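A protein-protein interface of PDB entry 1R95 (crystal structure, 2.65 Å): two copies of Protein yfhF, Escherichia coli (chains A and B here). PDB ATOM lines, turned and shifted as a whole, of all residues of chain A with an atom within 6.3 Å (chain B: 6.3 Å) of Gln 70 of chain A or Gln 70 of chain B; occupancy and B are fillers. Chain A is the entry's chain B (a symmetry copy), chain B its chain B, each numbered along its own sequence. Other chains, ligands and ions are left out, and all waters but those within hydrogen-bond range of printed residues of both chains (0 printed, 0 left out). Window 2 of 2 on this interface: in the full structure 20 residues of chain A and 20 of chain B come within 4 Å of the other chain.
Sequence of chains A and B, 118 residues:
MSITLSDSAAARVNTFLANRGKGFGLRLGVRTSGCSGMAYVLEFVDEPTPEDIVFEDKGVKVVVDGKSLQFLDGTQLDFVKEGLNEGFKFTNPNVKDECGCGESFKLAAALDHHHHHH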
ATOM      1  N   ASP A  65       0.159  30.336  24.590  1.00  0.00           N
ATOM      2  CA  ASP A  65       0.153  31.446  23.635  1.00  0.00           C
ATOM      3  C   ASP A  65       0.632  30.936  22.286  1.00  0.00           C
ATOM      4  O   ASP A  65       1.573  30.123  22.209  1.00  0.00           O
ATOM      5  CB  ASP A  65       1.073  32.567  24.110  1.00  0.00           C
ATOM      6  CG  ASP A  65       0.807  33.891  23.404  1.00  0.00           C
ATOM      7  OD1 ASP A  65       1.520  34.175  22.407  1.00  0.00           O
ATOM      8  OD2 ASP A  65      -0.075  34.716  23.784  1.00  0.00           O
ATOM      9  N   GLY A  66      -0.019  31.396  21.221  1.00  0.00           N
ATOM     10  CA  GLY A  66       0.261  30.912  19.878  1.00  0.00           C
ATOM     11  C   GLY A  66       1.695  31.170  19.475  1.00  0.00           C
ATOM     12  O   GLY A  66       2.357  30.306  18.891  1.00  0.00           O
ATOM     13  N   LYS A  67       2.175  32.357  19.828  1.00  0.00           N
ATOM     14  CA  LYS A  67       3.562  32.748  19.610  1.00  0.00           C
ATOM     15  C   LYS A  67       4.610  31.929  20.381  1.00  0.00           C
ATOM     16  O   LYS A  67       5.765  31.883  19.953  1.00  0.00           O
ATOM     17  CB  LYS A  67       3.744  34.257  19.873  1.00  0.00           C
ATOM     18  CG  LYS A  67       3.550  35.109  18.610  1.00  0.00           C
ATOM     19  CD  LYS A  67       3.143  36.546  18.904  1.00  0.00           C
ATOM     20  CE  LYS A  67       2.330  37.114  17.735  1.00  0.00           C
ATOM     21  NZ  LYS A  67       2.664  38.533  17.369  1.00  0.00           N
ATOM     22  N   SER A  68       4.231  31.287  21.491  1.00  0.00           N
ATOM     23  CA  SER A  68       5.195  30.484  22.271  1.00  0.00           C
ATOM     24  C   SER A  68       5.246  29.015  21.849  1.00  0.00           C
ATOM     25  O   SER A  68       6.034  28.232  22.390  1.00  0.00           O
ATOM     26  CB  SER A  68       4.912  30.561  23.777  1.00  0.00           C
ATOM     27  OG  SER A  68       5.099  31.864  24.290  1.00  0.00           O
ATOM     28  N   LEU A  69       4.410  28.640  20.891  1.00  0.00           N
ATOM     29  CA  LEU A  69       4.250  27.231  20.538  1.00  0.00           C
ATOM     30  C   LEU A  69       5.481  26.610  19.902  1.00  0.00           C
ATOM     31  O   LEU A  69       5.730  25.415  20.060  1.00  0.00           O
ATOM     32  CB  LEU A  69       3.040  27.024  19.632  1.00  0.00           C
ATOM     33  CG  LEU A  69       2.601  25.569  19.460  1.00  0.00           C
ATOM     34  CD1 LEU A  69       2.496  24.834  20.785  1.00  0.00           C
ATOM     35  CD2 LEU A  69       1.290  25.511  18.748  1.00  0.00           C
ATOM     36  N   GLN A  70       6.248  27.416  19.175  1.00  0.00           N
ATOM     37  CA  GLN A  70       7.488  26.939  18.554  1.00  0.00           C
ATOM     38  C   GLN A  70       8.472  26.420  19.603  1.00  0.00           C
ATOM     39  O   GLN A  70       9.088  25.376  19.400  1.00  0.00           O
ATOM     40  CB  GLN A  70       8.136  28.040  17.707  1.00  0.00           C
ATOM     41  CG  GLN A  70       8.326  29.378  18.446  1.00  0.00           C
ATOM     42  CD  GLN A  70       9.256  30.323  17.709  1.00  0.00           C
ATOM     43  OE1 GLN A  70       8.811  31.346  17.164  1.00  0.00           O
ATOM     44  NE2 GLN A  70      10.546  29.982  17.677  1.00  0.00           N
ATOM     45  N   PHE A  71       8.593  27.141  20.722  1.00  0.00           N
ATOM     46  CA  PHE A  71       9.478  26.740  21.820  1.00  0.00           C
ATOM     47  C   PHE A  71       8.969  25.529  22.620  1.00  0.00           C
ATOM     48  O   PHE A  71       9.772  24.715  23.079  1.00  0.00           O
ATOM     49  CB  PHE A  71       9.797  27.910  22.769  1.00  0.00           C
ATOM     50  CG  PHE A  71       9.899  29.251  22.080  1.00  0.00           C
ATOM     51  CD1 PHE A  71       8.812  30.136  22.075  1.00  0.00           C
ATOM     52  CD2 PHE A  71      11.081  29.638  21.436  1.00  0.00           C
ATOM     53  CE1 PHE A  71       8.890  31.375  21.436  1.00  0.00           C
ATOM     54  CE2 PHE A  71      11.171  30.882  20.793  1.00  0.00           C
ATOM     55  CZ  PHE A  71      10.071  31.751  20.789  1.00  0.00           C
ATOM     56  N   LEU A  72       7.655  25.389  22.777  1.00  0.00           N
ATOM     57  CA  LEU A  72       7.135  24.354  23.682  1.00  0.00           C
ATOM     58  C   LEU A  72       6.759  23.021  23.031  1.00  0.00           C
ATOM     59  O   LEU A  72       6.624  22.023  23.733  1.00  0.00           O
ATOM     60  CB  LEU A  72       5.989  24.893  24.537  1.00  0.00           C
ATOM     61  CG  LEU A  72       6.356  26.052  25.470  1.00  0.00           C
ATOM     62  CD1 LEU A  72       5.166  26.948  25.745  1.00  0.00           C
ATOM     63  CD2 LEU A  72       6.919  25.514  26.772  1.00  0.00           C
ATOM     64  N   ASP A  73       6.609  22.980  21.710  1.00  0.00           N
ATOM     65  CA  ASP A  73       6.218  21.734  21.048  1.00  0.00           C
ATOM     66  C   ASP A  73       7.192  20.570  21.290  1.00  0.00           C
ATOM     67  O   ASP A  73       8.406  20.707  21.108  1.00  0.00           O
ATOM     68  CB  ASP A  73       5.988  21.947  19.549  1.00  0.00           C
ATOM     69  CG  ASP A  73       4.739  21.214  19.030  1.00  0.00           C
ATOM     70  OD1 ASP A  73       4.314  21.491  17.881  1.00  0.00           O
ATOM     71  OD2 ASP A  73       4.114  20.350  19.699  1.00  0.00           O
ATOM     72  N   GLY A  74       6.646  19.429  21.707  1.00  0.00           N
ATOM     73  CA  GLY A  74       7.441  18.252  22.015  1.00  0.00           C
ATOM     74  C   GLY A  74       7.791  18.142  23.492  1.00  0.00           C
ATOM     75  O   GLY A  74       8.387  17.139  23.916  1.00  0.00           O
ATOM     76  N   ASN A  92      12.492  17.604  26.681  1.00  0.00           N
ATOM     77  CA  ASN A  92      12.330  17.497  25.242  1.00  0.00           C
ATOM     78  C   ASN A  92      13.286  16.420  24.732  1.00  0.00           C
ATOM     79  O   ASN A  92      14.467  16.396  25.113  1.00  0.00           O
ATOM     80  CB  ASN A  92      12.612  18.834  24.555  1.00  0.00           C
ATOM     81  CG  ASN A  92      11.663  19.113  23.413  1.00  0.00           C
ATOM     82  OD1 ASN A  92      11.551  18.322  22.477  1.00  0.00           O
ATOM     83  ND2 ASN A  92      10.973  20.248  23.480  1.00  0.00           N
ATOM     84  N   ASN A  94      14.023  16.304  21.406  1.00  0.00           N
ATOM     85  CA  ASN A  94      14.781  17.193  20.513  1.00  0.00           C
ATOM     86  C   ASN A  94      15.975  17.912  21.179  1.00  0.00           C
ATOM     87  O   ASN A  94      17.058  17.991  20.596  1.00  0.00           O
ATOM     88  CB  ASN A  94      13.832  18.220  19.867  1.00  0.00           C
ATOM     89  CG  ASN A  94      13.205  17.727  18.543  1.00  0.00           C
ATOM     90  OD1 ASN A  94      12.679  18.534  17.758  1.00  0.00           O
ATOM     91  ND2 ASN A  94      13.249  16.414  18.298  1.00  0.00           N
ATOM     92  N   ASP B  65      21.417  22.591  14.082  1.00  0.00           N
ATOM     93  CA  ASP B  65      20.854  21.239  14.064  1.00  0.00           C
ATOM     94  C   ASP B  65      19.378  21.325  13.710  1.00  0.00           C
ATOM     95  O   ASP B  65      18.664  22.234  14.174  1.00  0.00           O
ATOM     96  CB  ASP B  65      21.010  20.575  15.430  1.00  0.00           C
ATOM     97  CG  ASP B  65      20.832  19.063  15.377  1.00  0.00           C
ATOM     98  OD1 ASP B  65      19.696  18.598  15.648  1.00  0.00           O
ATOM     99  OD2 ASP B  65      21.773  18.262  15.095  1.00  0.00           O
ATOM    100  N   GLY B  66      18.920  20.394  12.878  1.00  0.00           N
ATOM    101  CA  GLY B  66      17.558  20.418  12.370  1.00  0.00           C
ATOM    102  C   GLY B  66      16.540  20.337  13.485  1.00  0.00           C
ATOM    103  O   GLY B  66      15.535  21.055  13.483  1.00  0.00           O
ATOM    104  N   LYS B  67      16.833  19.479  14.456  1.00  0.00           N
ATOM    105  CA  LYS B  67      16.022  19.332  15.657  1.00  0.00           C
ATOM    106  C   LYS B  67      15.958  20.569  16.567  1.00  0.00           C
ATOM    107  O   LYS B  67      14.999  20.699  17.332  1.00  0.00           O
ATOM    108  CB  LYS B  67      16.461  18.087  16.454  1.00  0.00           C
ATOM    109  CG  LYS B  67      15.684  16.823  16.058  1.00  0.00           C
ATOM    110  CD  LYS B  67      16.435  15.531  16.353  1.00  0.00           C
ATOM    111  CE  LYS B  67      15.995  14.431  15.380  1.00  0.00           C
ATOM    112  NZ  LYS B  67      15.814  13.077  16.006  1.00  0.00           N
ATOM    113  N   SER B  68      16.943  21.470  16.496  1.00  0.00           N
ATOM    114  CA  SER B  68      16.934  22.677  17.346  1.00  0.00           C
ATOM    115  C   SER B  68      16.252  23.878  16.689  1.00  0.00           C
ATOM    116  O   SER B  68      16.136  24.948  17.298  1.00  0.00           O
ATOM    117  CB  SER B  68      18.349  23.082  17.777  1.00  0.00           C
ATOM    118  OG  SER B  68      18.951  22.113  18.612  1.00  0.00           O
ATOM    119  N   LEU B  69      15.804  23.708  15.453  1.00  0.00           N
ATOM    120  CA  LEU B  69      15.300  24.835  14.670  1.00  0.00           C
ATOM    121  C   LEU B  69      14.011  25.431  15.206  1.00  0.00           C
ATOM    122  O   LEU B  69      13.767  26.628  15.057  1.00  0.00           O
ATOM    123  CB  LEU B  69      15.123  24.452  13.204  1.00  0.00           C
ATOM    124  CG  LEU B  69      14.903  25.627  12.250  1.00  0.00           C
ATOM    125  CD1 LEU B  69      15.909  26.745  12.465  1.00  0.00           C
ATOM    126  CD2 LEU B  69      14.970  25.156  10.836  1.00  0.00           C
ATOM    127  N   GLN B  70      13.178  24.597  15.822  1.00  0.00           N
ATOM    128  CA  GLN B  70      11.926  25.069  16.423  1.00  0.00           C
ATOM    129  C   GLN B  70      12.189  26.117  17.504  1.00  0.00           C
ATOM    130  O   GLN B  70      11.488  27.126  17.562  1.00  0.00           O
ATOM    131  CB  GLN B  70      11.116  23.899  16.993  1.00  0.00           C
ATOM    132  CG  GLN B  70      11.912  22.980  17.939  1.00  0.00           C
ATOM    133  CD  GLN B  70      11.016  22.050  18.735  1.00  0.00           C
ATOM    134  OE1 GLN B  70      11.003  20.831  18.495  1.00  0.00           O
ATOM    135  NE2 GLN B  70      10.258  22.617  19.676  1.00  0.00           N
ATOM    136  N   PHE B  71      13.208  25.881  18.335  1.00  0.00           N
ATOM    137  CA  PHE B  71      13.587  26.820  19.397  1.00  0.00           C
ATOM    138  C   PHE B  71      14.263  28.102  18.884  1.00  0.00           C
ATOM    139  O   PHE B  71      14.066  29.173  19.460  1.00  0.00           O
ATOM    140  CB  PHE B  71      14.456  26.154  20.481  1.00  0.00           C
ATOM    141  CG  PHE B  71      14.107  24.708  20.748  1.00  0.00           C
ATOM    142  CD1 PHE B  71      14.843  23.675  20.153  1.00  0.00           C
ATOM    143  CD2 PHE B  71      13.045  24.373  21.596  1.00  0.00           C
ATOM    144  CE1 PHE B  71      14.528  22.334  20.385  1.00  0.00           C
ATOM    145  CE2 PHE B  71      12.721  23.029  21.839  1.00  0.00           C
ATOM    146  CZ  PHE B  71      13.461  22.007  21.228  1.00  0.00           C
ATOM    147  N   LEU B  72      15.039  28.012  17.806  1.00  0.00           N
ATOM    148  CA  LEU B  72      15.844  29.169  17.391  1.00  0.00           C
ATOM    149  C   LEU B  72      15.220  30.077  16.329  1.00  0.00           C
ATOM    150  O   LEU B  72      15.666  31.207  16.161  1.00  0.00           O
ATOM    151  CB  LEU B  72      17.256  28.743  16.989  1.00  0.00           C
ATOM    152  CG  LEU B  72      18.086  28.092  18.102  1.00  0.00           C
ATOM    153  CD1 LEU B  72      19.111  27.126  17.545  1.00  0.00           C
ATOM    154  CD2 LEU B  72      18.771  29.160  18.934  1.00  0.00           C
ATOM    155  N   ASP B  73      14.186  29.615  15.629  1.00  0.00           N
ATOM    156  CA  ASP B  73      13.578  30.436  14.580  1.00  0.00           C
ATOM    157  C   ASP B  73      13.039  31.785  15.082  1.00  0.00           C
ATOM    158  O   ASP B  73      12.293  31.847  16.065  1.00  0.00           O
ATOM    159  CB  ASP B  73      12.491  29.663  13.828  1.00  0.00           C
ATOM    160  CG  ASP B  73      12.547  29.890  12.307  1.00  0.00           C
ATOM    161  OD1 ASP B  73      11.864  29.141  11.563  1.00  0.00           O
ATOM    162  OD2 ASP B  73      13.246  30.785  11.765  1.00  0.00           O
ATOM    163  N   GLY B  74      13.430  32.860  14.401  1.00  0.00           N
ATOM    164  CA  GLY B  74      13.035  34.207  14.778  1.00  0.00           C
ATOM    165  C   GLY B  74      14.064  34.904  15.657  1.00  0.00           C
ATOM    166  O   GLY B  74      13.903  36.091  15.978  1.00  0.00           O
ATOM    167  N   ASN B  92      14.200  37.497  20.737  1.00  0.00           N
ATOM    168  CA  ASN B  92      13.061  37.051  19.954  1.00  0.00           C
ATOM    169  C   ASN B  92      11.923  38.050  20.152  1.00  0.00           C
ATOM    170  O   ASN B  92      11.630  38.453  21.290  1.00  0.00           O
ATOM    171  CB  ASN B  92      12.621  35.647  20.371  1.00  0.00           C
ATOM    172  CG  ASN B  92      12.214  34.791  19.194  1.00  0.00           C
ATOM    173  OD1 ASN B  92      11.328  35.159  18.422  1.00  0.00           O
ATOM    174  ND2 ASN B  92      12.859  33.637  19.049  1.00  0.00           N
ATOM    175  N   ASN B  94       8.751  37.131  19.313  1.00  0.00           N
ATOM    176  CA  ASN B  94       7.802  36.161  19.880  1.00  0.00           C
ATOM    177  C   ASN B  94       7.893  35.989  21.413  1.00  0.00           C
ATOM    178  O   ASN B  94       6.869  35.935  22.095  1.00  0.00           O
ATOM    179  CB  ASN B  94       7.963  34.799  19.179  1.00  0.00           C
ATOM    180  CG  ASN B  94       7.079  34.650  17.919  1.00  0.00           C
ATOM    181  OD1 ASN B  94       6.861  33.528  17.434  1.00  0.00           O
ATOM    182  ND2 ASN B  94       6.580  35.771  17.387  1.00  0.00           N
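The backbone carbonyl oxygen (O) of Lys 67 of chain B lies close to the side-chain amide oxygen (OD1) of Asn 94 of chain A (3.2 Å).
O of Gln 70 of chain B lies within hydrogen-bond range of NE2 of Gln 70 of chain A, 3.0 Å away.
The side-chain amide nitrogen (NE2) of Gln 70 of chain B lies within hydrogen-bond range of the backbone carbonyl oxygen (O) of Asp 73 of chain A (3.0 Å).
The side-chain amide oxygen (OE1) of Gln 70 of chain B sits close to the side-chain amide oxygen (OD1) of Asn 94 of chain A, 2.9 Å away.
O of Asp 73 of chain B sits at hydrogen-bond distance from NE2 of Gln 70 of chain A, 3.0 Å away.
The backbone carbonyl oxygen (O) of Lys 67 of chain A lies close to the side-chain amide oxygen (OD1) of Asn 94 of chain B.
OD1 of Asn 94 of chain B sits close to OE1 of Gln 70 of chain A, at 2.9 Å.
The backbone NH (N) of Lys 67 of chain B is in hydrogen-bond range of the side-chain carboxylate (OD1) of Asp 65 of chain B (3.2 Å).
The backbone NH of Asn 94 of chain B sits at hydrogen-bond distance from the side-chain amide oxygen of Asn 92 of chain B.
N of Lys 67 of chain A sits at hydrogen-bond distance from OD1 of Asp 65 of chain A (3.2 Å).
N of Asn 94 of chain A is in hydrogen-bond range of OD1 of Asn 92 of chain A, 3.4 Å away.
Phe 71 of chain A touches Phe 71 of chain B.
Asn 92 of chain B touches Phe 71 of chain A.
ND2 of Asn 92 of chain A touches CE2 of Phe 71 of chain B, 3.7 Å away.
Of chain B, only Gln 70, Asp 73 and Asn 94 come within 4 Å of Gln 70 of chain A.
Of chain A, only Gln 70, Asp 73 and Asn 94 come within 4 Å of Gln 70 of chain B.
Of the printed residues of chain B, Lys 67 of chain A touches Asn 94.
Of the printed residues of chain B, Asn 92 of chain A touches Phe 71.
Printed residues of chain A within 4 Å of Asn 92 of chain B: Phe 71.
Of the printed residues of chain A, Asn 94 of chain B touches Lys 67 and Gln 70.
Printed residues of chain A within 4 Å of Asp 73 of chain B: Gln 70.
Ser 68 of chain A touches none of the printed residues of chain B.
The nearest residue of chain B that does not touch Gln 70 of chain A is Phe 71 of chain B (4.03 Å).
The nearest residue of chain A that does not touch Gln 70 of chain B is Phe 71 of chain A (4.03 Å).
Of the 12 printed residues of chain B, 6 touch a printed residue of chain A.
Printed residues of chain B that touch a printed residue of chain A: Lys 67, Gln 70, Phe 71, Asp 73, Asn 92 and Asn 94.
Hydrophobic or aromatic side chains of chain B within 4 Å of the printed part of chain A: Phe 71.
Of the 12 printed residues of chain A, 6 touch a printed residue of chain B.
Among the printed residues, 10 pairs touch across the chains.
Lys 67 of chain A touches Asn 94 of chain B, and with the chains exchanged Asn 94 of chain A touches Lys 67 of chain B.
Gln 70 of chain A touches Asn 94 of chain B, and with the chains exchanged Asn 94 of chain A touches Gln 70 of chain B.
Phe 71 of chain A touches its own counterpart, Phe 71 of chain B.
Phe 71 of chain A touches Asn 92 of chain B, and with the chains exchanged Asn 92 of chain A touches Phe 71 of chain B.
Positions printed for both chains: 65, 66, 67, 68, 69, 70, 71, 72, 73, 74, 92 and 94.
Of the 10 pairs that touch across the chains among the printed residues, 10 have their exchanged pair printed and touching as well.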
